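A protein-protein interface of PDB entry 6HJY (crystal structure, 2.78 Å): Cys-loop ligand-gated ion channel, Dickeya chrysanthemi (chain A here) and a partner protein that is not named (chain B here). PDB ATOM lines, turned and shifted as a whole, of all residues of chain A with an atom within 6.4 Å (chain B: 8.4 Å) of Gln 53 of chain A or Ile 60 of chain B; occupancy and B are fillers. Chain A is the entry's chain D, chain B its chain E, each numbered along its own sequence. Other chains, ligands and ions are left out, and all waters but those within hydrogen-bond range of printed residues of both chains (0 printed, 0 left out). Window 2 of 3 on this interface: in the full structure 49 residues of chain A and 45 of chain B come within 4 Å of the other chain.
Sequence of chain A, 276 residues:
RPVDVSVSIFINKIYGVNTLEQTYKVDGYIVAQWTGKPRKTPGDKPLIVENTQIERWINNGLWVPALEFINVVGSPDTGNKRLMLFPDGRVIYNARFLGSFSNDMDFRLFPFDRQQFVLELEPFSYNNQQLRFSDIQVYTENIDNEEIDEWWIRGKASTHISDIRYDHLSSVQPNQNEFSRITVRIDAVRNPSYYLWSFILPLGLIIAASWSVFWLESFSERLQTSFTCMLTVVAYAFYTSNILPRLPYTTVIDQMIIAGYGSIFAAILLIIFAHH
The guanidinium group (NH2) of Arg 56 of chain A is in hydrogen-bond range of the backbone carbonyl oxygen (O) of Asn 61 of chain B. OE1 of Glu 50 of chain A lies within hydrogen-bond range of N of Ala 68 of chain B (3.2 Å). The side-chain hydroxyl of Thr 52 of chain A sits at hydrogen-bond distance from the side-chain carboxylate of Glu 57 of chain B (2.7 Å). The side-chain carboxylate (OE2) of Glu 57 of chain B lies within hydrogen-bond range of the side-chain amide nitrogen (NE2) of Gln 53 of chain A, at 3.2 Å. The side-chain amide nitrogen (NE2) of Gln 53 of chain A lies within hydrogen-bond range of the side-chain amide oxygen (OD1) of Asn 61 of chain B, at 2.7 Å.
OE2 of Glu 57 of chain B lies close to OD1 of Asn 61 of chain B. The guanidinium group (NE) of Arg 56 of chain A is in hydrogen-bond range of the side-chain amide oxygen (OE1) of Gln 53 of chain A.
Among the printed residues, pairs that only touch across the chains: Gln 53 of chain A with Ile 60 of chain B (3.7 Å) and Asn 51 of chain A with Ala 68 of chain B (3.8 Å).
Gln 53 of chain A touches just these residues of chain B: Glu 57 (3.2 Å), Ile 60 (3.7 Å) and Asn 61 (2.7 Å). Of the printed residues of chain B, Arg 56 of chain A touches Asn 61 (3.0 Å). Of the printed residues of chain B, Thr 52 of chain A touches Glu 57 (2.7 Å). Of the printed residues of chain B, Asn 51 of chain A touches Ala 68. Of the printed residues of chain A, Ala 68 of chain B touches Glu 50 and Asn 51. Of the printed residues of chain B, Glu 50 of chain A touches Ala 68 (3.2 Å). Arg 58 of chain B touches none of the printed residues of chain A. Glu 55 of chain A touches none of the printed residues of chain B. The nearest residue of chain B that does not touch Gln 53 of chain A is Asn 62 of chain B (6.0 Å). The nearest printed residue of chain A that does not touch Asn 61 of chain B is Thr 52 of chain A (5.2 Å).
Of the 10 printed residues of chain A, 5 touch a printed residue of chain B. Of the 20 printed residues of chain B, 4 touch a printed residue of chain A. Printed residues of chain B that touch a printed residue of chain A: Glu 57, Ile 60, Asn 61 and Ala 68. Hydrophobic or aromatic side chains of chain B that line the printed part of chain A: Ile 60 and Ala 68. Along chain B the printed residues that touch a printed residue of chain A span positions 57 to 68. Among the printed residues, 7 pairs touch across the chains.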
ATOM      1  N   VAL A  49     -24.029  -1.131   4.879  1.00  0.00           N
ATOM      2  CA  VAL A  49     -23.877  -2.581   5.106  1.00  0.00           C
ATOM      3  C   VAL A  49     -24.703  -3.282   4.003  1.00  0.00           C
ATOM      4  O   VAL A  49     -25.926  -3.177   3.993  1.00  0.00           O
ATOM      5  CB  VAL A  49     -24.297  -3.034   6.535  1.00  0.00           C
ATOM      6  CG1 VAL A  49     -23.942  -4.491   6.761  1.00  0.00           C
ATOM      7  CG2 VAL A  49     -23.646  -2.175   7.617  1.00  0.00           C
ATOM      8  N   GLU A  50     -24.039  -3.899   3.016  1.00  0.00           N
ATOM      9  CA  GLU A  50     -24.758  -4.536   1.919  1.00  0.00           C
ATOM     10  C   GLU A  50     -24.902  -6.037   2.036  1.00  0.00           C
ATOM     11  O   GLU A  50     -24.118  -6.721   2.692  1.00  0.00           O
ATOM     12  CB  GLU A  50     -24.087  -4.233   0.571  1.00  0.00           C
ATOM     13  CG  GLU A  50     -24.269  -2.821   0.051  1.00  0.00           C
ATOM     14  CD  GLU A  50     -23.475  -2.504  -1.201  1.00  0.00           C
ATOM     15  OE1 GLU A  50     -22.441  -3.164  -1.431  1.00  0.00           O
ATOM     16  OE2 GLU A  50     -23.878  -1.595  -1.956  1.00  0.00           O
ATOM     17  N   ASN A  51     -25.943  -6.531   1.370  1.00  0.00           N
ATOM     18  CA  ASN A  51     -26.373  -7.889   1.120  1.00  0.00           C
ATOM     19  C   ASN A  51     -26.070  -8.901   2.268  1.00  0.00           C
ATOM     20  O   ASN A  51     -26.784  -8.891   3.275  1.00  0.00           O
ATOM     21  CB  ASN A  51     -25.773  -8.367  -0.216  1.00  0.00           C
ATOM     22  CG  ASN A  51     -26.277  -7.572  -1.408  1.00  0.00           C
ATOM     23  OD1 ASN A  51     -27.473  -7.500  -1.674  1.00  0.00           O
ATOM     24  ND2 ASN A  51     -25.390  -6.895  -2.113  1.00  0.00           N
ATOM     25  N   THR A  52     -25.025  -9.728   2.113  1.00  0.00           N
ATOM     26  CA  THR A  52     -24.586 -10.777   3.039  1.00  0.00           C
ATOM     27  C   THR A  52     -23.964 -10.239   4.339  1.00  0.00           C
ATOM     28  O   THR A  52     -23.927 -10.986   5.317  1.00  0.00           O
ATOM     29  CB  THR A  52     -23.624 -11.728   2.304  1.00  0.00           C
ATOM     30  OG1 THR A  52     -22.694 -10.962   1.545  1.00  0.00           O
ATOM     31  CG2 THR A  52     -24.345 -12.736   1.402  1.00  0.00           C
ATOM     32  N   GLN A  53     -23.490  -8.969   4.356  1.00  0.00           N
ATOM     33  CA  GLN A  53     -22.890  -8.341   5.532  1.00  0.00           C
ATOM     34  C   GLN A  53     -23.906  -8.039   6.616  1.00  0.00           C
ATOM     35  O   GLN A  53     -23.572  -8.083   7.803  1.00  0.00           O
ATOM     36  CB  GLN A  53     -22.087  -7.088   5.151  1.00  0.00           C
ATOM     37  CG  GLN A  53     -20.707  -7.375   4.568  1.00  0.00           C
ATOM     38  CD  GLN A  53     -20.003  -8.443   5.357  1.00  0.00           C
ATOM     39  OE1 GLN A  53     -19.586  -8.224   6.501  1.00  0.00           O
ATOM     40  NE2 GLN A  53     -20.020  -9.658   4.826  1.00  0.00           N
ATOM     41  N   ILE A  54     -25.164  -7.747   6.197  1.00  0.00           N
ATOM     42  CA  ILE A  54     -26.315  -7.472   7.072  1.00  0.00           C
ATOM     43  C   ILE A  54     -26.563  -8.651   8.000  1.00  0.00           C
ATOM     44  O   ILE A  54     -26.737  -8.453   9.207  1.00  0.00           O
ATOM     45  CB  ILE A  54     -27.614  -7.125   6.278  1.00  0.00           C
ATOM     46  CG1 ILE A  54     -27.388  -5.926   5.344  1.00  0.00           C
ATOM     47  CG2 ILE A  54     -28.808  -6.884   7.248  1.00  0.00           C
ATOM     48  CD1 ILE A  54     -28.455  -5.679   4.382  1.00  0.00           C
ATOM     49  N   GLU A  55     -26.551  -9.889   7.437  1.00  0.00           N
ATOM     50  CA  GLU A  55     -26.776 -11.115   8.210  1.00  0.00           C
ATOM     51  C   GLU A  55     -25.825 -11.195   9.406  1.00  0.00           C
ATOM     52  O   GLU A  55     -26.278 -11.535  10.499  1.00  0.00           O
ATOM     53  CB  GLU A  55     -26.769 -12.403   7.342  1.00  0.00           C
ATOM     54  CG  GLU A  55     -27.494 -13.596   7.972  1.00  0.00           C
ATOM     55  CD  GLU A  55     -28.800 -13.276   8.686  1.00  0.00           C
ATOM     56  OE1 GLU A  55     -29.738 -12.774   8.022  1.00  0.00           O
ATOM     57  OE2 GLU A  55     -28.892 -13.536   9.908  1.00  0.00           O
ATOM     58  N   ARG A  56     -24.569 -10.729   9.225  1.00  0.00           N
ATOM     59  CA  ARG A  56     -23.541 -10.665  10.270  1.00  0.00           C
ATOM     60  C   ARG A  56     -23.933  -9.674  11.387  1.00  0.00           C
ATOM     61  O   ARG A  56     -23.757  -9.990  12.568  1.00  0.00           O
ATOM     62  CB  ARG A  56     -22.145 -10.359   9.686  1.00  0.00           C
ATOM     63  CG  ARG A  56     -21.687 -11.330   8.587  1.00  0.00           C
ATOM     64  CD  ARG A  56     -20.197 -11.665   8.662  1.00  0.00           C
ATOM     65  NE  ARG A  56     -19.360 -10.466   8.544  1.00  0.00           N
ATOM     66  CZ  ARG A  56     -18.403 -10.121   9.402  1.00  0.00           C
ATOM     67  NH1 ARG A  56     -18.139 -10.880  10.457  1.00  0.00           N
ATOM     68  NH2 ARG A  56     -17.696  -9.016   9.203  1.00  0.00           N
ATOM     69  N   TRP A  57     -24.510  -8.505  11.011  1.00  0.00           N
ATOM     70  CA  TRP A  57     -24.988  -7.482  11.951  1.00  0.00           C
ATOM     71  C   TRP A  57     -26.195  -7.976  12.745  1.00  0.00           C
ATOM     72  O   TRP A  57     -26.306  -7.657  13.932  1.00  0.00           O
ATOM     73  CB  TRP A  57     -25.366  -6.199  11.207  1.00  0.00           C
ATOM     74  CG  TRP A  57     -24.183  -5.344  10.913  1.00  0.00           C
ATOM     75  CD1 TRP A  57     -23.279  -5.517   9.909  1.00  0.00           C
ATOM     76  CD2 TRP A  57     -23.703  -4.256  11.706  1.00  0.00           C
ATOM     77  NE1 TRP A  57     -22.295  -4.559   9.986  1.00  0.00           N
ATOM     78  CE2 TRP A  57     -22.528  -3.773  11.086  1.00  0.00           C
ATOM     79  CE3 TRP A  57     -24.168  -3.617  12.867  1.00  0.00           C
ATOM     80  CZ2 TRP A  57     -21.805  -2.692  11.598  1.00  0.00           C
ATOM     81  CZ3 TRP A  57     -23.464  -2.534  13.362  1.00  0.00           C
ATOM     82  CH2 TRP A  57     -22.305  -2.069  12.722  1.00  0.00           C
ATOM     83  N   ILE A  58     -27.107  -8.746  12.089  1.00  0.00           N
ATOM     84  CA  ILE A  58     -28.312  -9.299  12.727  1.00  0.00           C
ATOM     85  C   ILE A  58     -27.913 -10.326  13.794  1.00  0.00           C
ATOM     86  O   ILE A  58     -28.365 -10.210  14.935  1.00  0.00           O
ATOM     87  CB  ILE A  58     -29.372  -9.821  11.704  1.00  0.00           C
ATOM     88  CG1 ILE A  58     -29.997  -8.639  10.939  1.00  0.00           C
ATOM     89  CG2 ILE A  58     -30.479 -10.661  12.390  1.00  0.00           C
ATOM     90  CD1 ILE A  58     -30.807  -8.979   9.711  1.00  0.00           C
ATOM     91  N   VAL B  51      -9.221 -14.664  -6.468  1.00  0.00           N
ATOM     92  CA  VAL B  51     -10.188 -15.111  -5.462  1.00  0.00           C
ATOM     93  C   VAL B  51     -11.499 -15.289  -6.221  1.00  0.00           C
ATOM     94  O   VAL B  51     -11.958 -14.355  -6.881  1.00  0.00           O
ATOM     95  CB  VAL B  51     -10.373 -14.100  -4.297  1.00  0.00           C
ATOM     96  CG1 VAL B  51     -11.168 -14.717  -3.166  1.00  0.00           C
ATOM     97  CG2 VAL B  51      -9.042 -13.563  -3.772  1.00  0.00           C
ATOM     98  N   ASN B  53     -15.661 -17.017  -6.573  1.00  0.00           N
ATOM     99  CA  ASN B  53     -16.954 -17.507  -6.128  1.00  0.00           C
ATOM    100  C   ASN B  53     -17.198 -17.281  -4.614  1.00  0.00           C
ATOM    101  O   ASN B  53     -17.226 -16.125  -4.189  1.00  0.00           O
ATOM    102  CB  ASN B  53     -17.188 -18.969  -6.558  1.00  0.00           C
ATOM    103  CG  ASN B  53     -17.288 -19.083  -8.070  1.00  0.00           C
ATOM    104  OD1 ASN B  53     -17.943 -18.276  -8.727  1.00  0.00           O
ATOM    105  ND2 ASN B  53     -16.606 -20.043  -8.674  1.00  0.00           N
ATOM    106  N   THR B  54     -17.383 -18.350  -3.833  1.00  0.00           N
ATOM    107  CA  THR B  54     -17.692 -18.287  -2.399  1.00  0.00           C
ATOM    108  C   THR B  54     -16.555 -17.667  -1.543  1.00  0.00           C
ATOM    109  O   THR B  54     -16.830 -17.233  -0.422  1.00  0.00           O
ATOM    110  CB  THR B  54     -18.075 -19.688  -1.904  1.00  0.00           C
ATOM    111  OG1 THR B  54     -16.914 -20.499  -1.923  1.00  0.00           O
ATOM    112  CG2 THR B  54     -19.208 -20.342  -2.746  1.00  0.00           C
ATOM    113  N   GLN B  55     -15.299 -17.643  -2.056  1.00  0.00           N
ATOM    114  CA  GLN B  55     -14.149 -17.083  -1.336  1.00  0.00           C
ATOM    115  C   GLN B  55     -14.167 -15.557  -1.294  1.00  0.00           C
ATOM    116  O   GLN B  55     -13.570 -14.984  -0.382  1.00  0.00           O
ATOM    117  CB  GLN B  55     -12.821 -17.608  -1.898  1.00  0.00           C
ATOM    118  CG  GLN B  55     -12.658 -19.134  -1.814  1.00  0.00           C
ATOM    119  CD  GLN B  55     -12.939 -19.713  -0.449  1.00  0.00           C
ATOM    120  OE1 GLN B  55     -12.398 -19.270   0.564  1.00  0.00           O
ATOM    121  NE2 GLN B  55     -13.730 -20.764  -0.426  1.00  0.00           N
ATOM    122  N   ILE B  56     -14.887 -14.901  -2.258  1.00  0.00           N
ATOM    123  CA  ILE B  56     -15.073 -13.440  -2.350  1.00  0.00           C
ATOM    124  C   ILE B  56     -15.756 -12.978  -1.067  1.00  0.00           C
ATOM    125  O   ILE B  56     -15.332 -11.992  -0.459  1.00  0.00           O
ATOM    126  CB  ILE B  56     -15.889 -13.015  -3.623  1.00  0.00           C
ATOM    127  CG1 ILE B  56     -15.219 -13.553  -4.921  1.00  0.00           C
ATOM    128  CG2 ILE B  56     -16.111 -11.476  -3.657  1.00  0.00           C
ATOM    129  CD1 ILE B  56     -15.665 -13.013  -6.243  1.00  0.00           C
ATOM    130  N   GLU B  57     -16.790 -13.743  -0.640  1.00  0.00           N
ATOM    131  CA  GLU B  57     -17.561 -13.517   0.575  1.00  0.00           C
ATOM    132  C   GLU B  57     -16.688 -13.529   1.814  1.00  0.00           C
ATOM    133  O   GLU B  57     -16.850 -12.656   2.665  1.00  0.00           O
ATOM    134  CB  GLU B  57     -18.732 -14.509   0.697  1.00  0.00           C
ATOM    135  CG  GLU B  57     -19.873 -14.008   1.571  1.00  0.00           C
ATOM    136  CD  GLU B  57     -20.184 -12.528   1.414  1.00  0.00           C
ATOM    137  OE1 GLU B  57     -20.593 -12.124   0.301  1.00  0.00           O
ATOM    138  OE2 GLU B  57     -20.054 -11.774   2.407  1.00  0.00           O
ATOM    139  N   ARG B  58     -15.694 -14.440   1.854  1.00  0.00           N
ATOM    140  CA  ARG B  58     -14.722 -14.535   2.950  1.00  0.00           C
ATOM    141  C   ARG B  58     -13.851 -13.277   3.045  1.00  0.00           C
ATOM    142  O   ARG B  58     -13.562 -12.821   4.151  1.00  0.00           O
ATOM    143  CB  ARG B  58     -13.866 -15.804   2.832  1.00  0.00           C
ATOM    144  CG  ARG B  58     -14.685 -17.068   3.071  1.00  0.00           C
ATOM    145  CD  ARG B  58     -13.838 -18.326   3.144  1.00  0.00           C
ATOM    146  NE  ARG B  58     -12.940 -18.334   4.300  1.00  0.00           N
ATOM    147  CZ  ARG B  58     -11.619 -18.475   4.234  1.00  0.00           C
ATOM    148  NH1 ARG B  58     -11.015 -18.622   3.061  1.00  0.00           N
ATOM    149  NH2 ARG B  58     -10.890 -18.479   5.343  1.00  0.00           N
ATOM    150  N   TRP B  59     -13.476 -12.699   1.888  1.00  0.00           N
ATOM    151  CA  TRP B  59     -12.682 -11.473   1.801  1.00  0.00           C
ATOM    152  C   TRP B  59     -13.485 -10.256   2.218  1.00  0.00           C
ATOM    153  O   TRP B  59     -12.925  -9.355   2.840  1.00  0.00           O
ATOM    154  CB  TRP B  59     -12.117 -11.287   0.388  1.00  0.00           C
ATOM    155  CG  TRP B  59     -10.875 -12.089   0.163  1.00  0.00           C
ATOM    156  CD1 TRP B  59     -10.794 -13.435  -0.039  1.00  0.00           C
ATOM    157  CD2 TRP B  59      -9.530 -11.606   0.200  1.00  0.00           C
ATOM    158  NE1 TRP B  59      -9.480 -13.819  -0.159  1.00  0.00           N
ATOM    159  CE2 TRP B  59      -8.680 -12.714  -0.018  1.00  0.00           C
ATOM    160  CE3 TRP B  59      -8.957 -10.336   0.379  1.00  0.00           C
ATOM    161  CZ2 TRP B  59      -7.287 -12.594  -0.049  1.00  0.00           C
ATOM    162  CZ3 TRP B  59      -7.577 -10.219   0.353  1.00  0.00           C
ATOM    163  CH2 TRP B  59      -6.757 -11.332   0.125  1.00  0.00           C
ATOM    164  N   ILE B  60     -14.795 -10.233   1.887  1.00  0.00           N
ATOM    165  CA  ILE B  60     -15.709  -9.140   2.222  1.00  0.00           C
ATOM    166  C   ILE B  60     -15.942  -9.101   3.739  1.00  0.00           C
ATOM    167  O   ILE B  60     -15.841  -8.022   4.335  1.00  0.00           O
ATOM    168  CB  ILE B  60     -17.014  -9.193   1.374  1.00  0.00           C
ATOM    169  CG1 ILE B  60     -16.702  -8.863  -0.109  1.00  0.00           C
ATOM    170  CG2 ILE B  60     -18.105  -8.254   1.935  1.00  0.00           C
ATOM    171  CD1 ILE B  60     -17.790  -9.220  -1.138  1.00  0.00           C
ATOM    172  N   ASN B  61     -16.191 -10.282   4.364  1.00  0.00           N
ATOM    173  CA  ASN B  61     -16.374 -10.424   5.816  1.00  0.00           C
ATOM    174  C   ASN B  61     -15.121  -9.893   6.536  1.00  0.00           C
ATOM    175  O   ASN B  61     -15.229  -9.254   7.586  1.00  0.00           O
ATOM    176  CB  ASN B  61     -16.606 -11.892   6.217  1.00  0.00           C
ATOM    177  CG  ASN B  61     -17.802 -12.603   5.619  1.00  0.00           C
ATOM    178  OD1 ASN B  61     -18.790 -12.005   5.195  1.00  0.00           O
ATOM    179  ND2 ASN B  61     -17.742 -13.930   5.608  1.00  0.00           N
ATOM    180  N   ASN B  62     -13.938 -10.120   5.930  1.00  0.00           N
ATOM    181  CA  ASN B  62     -12.647  -9.694   6.454  1.00  0.00           C
ATOM    182  C   ASN B  62     -12.292  -8.221   6.119  1.00  0.00           C
ATOM    183  O   ASN B  62     -11.194  -7.775   6.456  1.00  0.00           O
ATOM    184  CB  ASN B  62     -11.543 -10.663   6.031  1.00  0.00           C
ATOM    185  CG  ASN B  62     -11.344 -11.776   7.031  1.00  0.00           C
ATOM    186  OD1 ASN B  62     -10.558 -11.654   7.970  1.00  0.00           O
ATOM    187  ND2 ASN B  62     -12.064 -12.878   6.870  1.00  0.00           N
ATOM    188  N   GLY B  63     -13.227  -7.480   5.521  1.00  0.00           N
ATOM    189  CA  GLY B  63     -13.040  -6.054   5.262  1.00  0.00           C
ATOM    190  C   GLY B  63     -12.796  -5.559   3.848  1.00  0.00           C
ATOM    191  O   GLY B  63     -12.611  -4.353   3.671  1.00  0.00           O
ATOM    192  N   LEU B  64     -12.794  -6.450   2.835  1.00  0.00           N
ATOM    193  CA  LEU B  64     -12.578  -6.017   1.446  1.00  0.00           C
ATOM    194  C   LEU B  64     -13.815  -5.307   0.876  1.00  0.00           C
ATOM    195  O   LEU B  64     -14.937  -5.806   1.007  1.00  0.00           O
ATOM    196  CB  LEU B  64     -12.135  -7.192   0.552  1.00  0.00           C
ATOM    197  CG  LEU B  64     -11.824  -6.885  -0.916  1.00  0.00           C
ATOM    198  CD1 LEU B  64     -10.486  -6.174  -1.080  1.00  0.00           C
ATOM    199  CD2 LEU B  64     -11.820  -8.144  -1.723  1.00  0.00           C
ATOM    200  N   TRP B  65     -13.596  -4.123   0.277  1.00  0.00           N
ATOM    201  CA  TRP B  65     -14.648  -3.303  -0.308  1.00  0.00           C
ATOM    202  C   TRP B  65     -14.959  -3.722  -1.741  1.00  0.00           C
ATOM    203  O   TRP B  65     -14.149  -3.506  -2.647  1.00  0.00           O
ATOM    204  CB  TRP B  65     -14.288  -1.813  -0.221  1.00  0.00           C
ATOM    205  CG  TRP B  65     -15.390  -0.889  -0.656  1.00  0.00           C
ATOM    206  CD1 TRP B  65     -16.522  -0.578   0.039  1.00  0.00           C
ATOM    207  CD2 TRP B  65     -15.445  -0.136  -1.874  1.00  0.00           C
ATOM    208  NE1 TRP B  65     -17.284   0.320  -0.674  1.00  0.00           N
ATOM    209  CE2 TRP B  65     -16.644   0.614  -1.850  1.00  0.00           C
ATOM    210  CE3 TRP B  65     -14.592  -0.016  -2.988  1.00  0.00           C
ATOM    211  CZ2 TRP B  65     -17.012   1.473  -2.894  1.00  0.00           C
ATOM    212  CZ3 TRP B  65     -14.954   0.842  -4.019  1.00  0.00           C
ATOM    213  CH2 TRP B  65     -16.146   1.579  -3.965  1.00  0.00           C
ATOM    214  N   VAL B  66     -16.117  -4.373  -1.930  1.00  0.00           N
ATOM    215  CA  VAL B  66     -16.610  -4.817  -3.235  1.00  0.00           C
ATOM    216  C   VAL B  66     -18.015  -4.205  -3.359  1.00  0.00           C
ATOM    217  O   VAL B  66     -18.966  -4.753  -2.793  1.00  0.00           O
ATOM    218  CB  VAL B  66     -16.601  -6.366  -3.427  1.00  0.00           C
ATOM    219  CG1 VAL B  66     -16.983  -6.740  -4.856  1.00  0.00           C
ATOM    220  CG2 VAL B  66     -15.242  -6.972  -3.070  1.00  0.00           C
ATOM    221  N   PRO B  67     -18.157  -3.026  -4.006  1.00  0.00           N
ATOM    222  CA  PRO B  67     -19.488  -2.399  -4.087  1.00  0.00           C
ATOM    223  C   PRO B  67     -20.472  -3.200  -4.926  1.00  0.00           C
ATOM    224  O   PRO B  67     -20.057  -3.892  -5.858  1.00  0.00           O
ATOM    225  CB  PRO B  67     -19.198  -1.038  -4.717  1.00  0.00           C
ATOM    226  CG  PRO B  67     -17.943  -1.239  -5.493  1.00  0.00           C
ATOM    227  CD  PRO B  67     -17.131  -2.221  -4.701  1.00  0.00           C
ATOM    228  N   ALA B  68     -21.770  -3.119  -4.579  1.00  0.00           N
ATOM    229  CA  ALA B  68     -22.829  -3.805  -5.317  1.00  0.00           C
ATOM    230  C   ALA B  68     -23.281  -2.911  -6.452  1.00  0.00           C
ATOM    231  O   ALA B  68     -23.678  -1.765  -6.220  1.00  0.00           O
ATOM    232  CB  ALA B  68     -23.994  -4.149  -4.403  1.00  0.00           C
ATOM    233  N   LYS B  83     -17.769 -15.870 -10.691  1.00  0.00           N
ATOM    234  CA  LYS B  83     -17.290 -14.507 -10.361  1.00  0.00           C
ATOM    235  C   LYS B  83     -15.959 -14.597  -9.672  1.00  0.00           C
ATOM    236  O   LYS B  83     -15.737 -15.538  -8.927  1.00  0.00           O
ATOM    237  CB  LYS B  83     -18.345 -13.707  -9.533  1.00  0.00           C
ATOM    238  CG  LYS B  83     -18.713 -14.304  -8.170  1.00  0.00           C
ATOM    239  CD  LYS B  83     -19.692 -13.420  -7.411  1.00  0.00           C
ATOM    240  CE  LYS B  83     -19.917 -13.954  -6.011  1.00  0.00           C
ATOM    241  NZ  LYS B  83     -20.870 -13.110  -5.235  1.00  0.00           N
ATOM    242  N   LEU B  85     -12.217 -12.082  -8.408  1.00  0.00           N
ATOM    243  CA  LEU B  85     -11.528 -10.869  -7.965  1.00  0.00           C
ATOM    244  C   LEU B  85     -10.060 -11.054  -8.239  1.00  0.00           C
ATOM    245  O   LEU B  85      -9.493 -12.105  -7.913  1.00  0.00           O
ATOM    246  CB  LEU B  85     -11.737 -10.557  -6.473  1.00  0.00           C
ATOM    247  CG  LEU B  85     -12.999  -9.791  -6.131  1.00  0.00           C
ATOM    248  CD1 LEU B  85     -13.169  -9.691  -4.657  1.00  0.00           C
ATOM    249  CD2 LEU B  85     -13.012  -8.400  -6.727  1.00  0.00           C
ATOM    250  N   TYR B  95     -13.128  -7.017 -10.771  1.00  0.00           N
ATOM    251  CA  TYR B  95     -14.263  -7.899 -10.556  1.00  0.00           C
ATOM    252  C   TYR B  95     -14.859  -8.309 -11.898  1.00  0.00           C
ATOM    253  O   TYR B  95     -15.302  -7.454 -12.664  1.00  0.00           O
ATOM    254  CB  TYR B  95     -15.324  -7.232  -9.653  1.00  0.00           C
ATOM    255  CG  TYR B  95     -16.655  -7.966  -9.605  1.00  0.00           C
ATOM    256  CD1 TYR B  95     -17.729  -7.560 -10.396  1.00  0.00           C
ATOM    257  CD2 TYR B  95     -16.839  -9.066  -8.767  1.00  0.00           C
ATOM    258  CE1 TYR B  95     -18.949  -8.237 -10.366  1.00  0.00           C
ATOM    259  CE2 TYR B  95     -18.059  -9.747  -8.724  1.00  0.00           C
ATOM    260  CZ  TYR B  95     -19.112  -9.324  -9.519  1.00  0.00           C
ATOM    261  OH  TYR B  95     -20.312  -9.987  -9.468  1.00  0.00           O
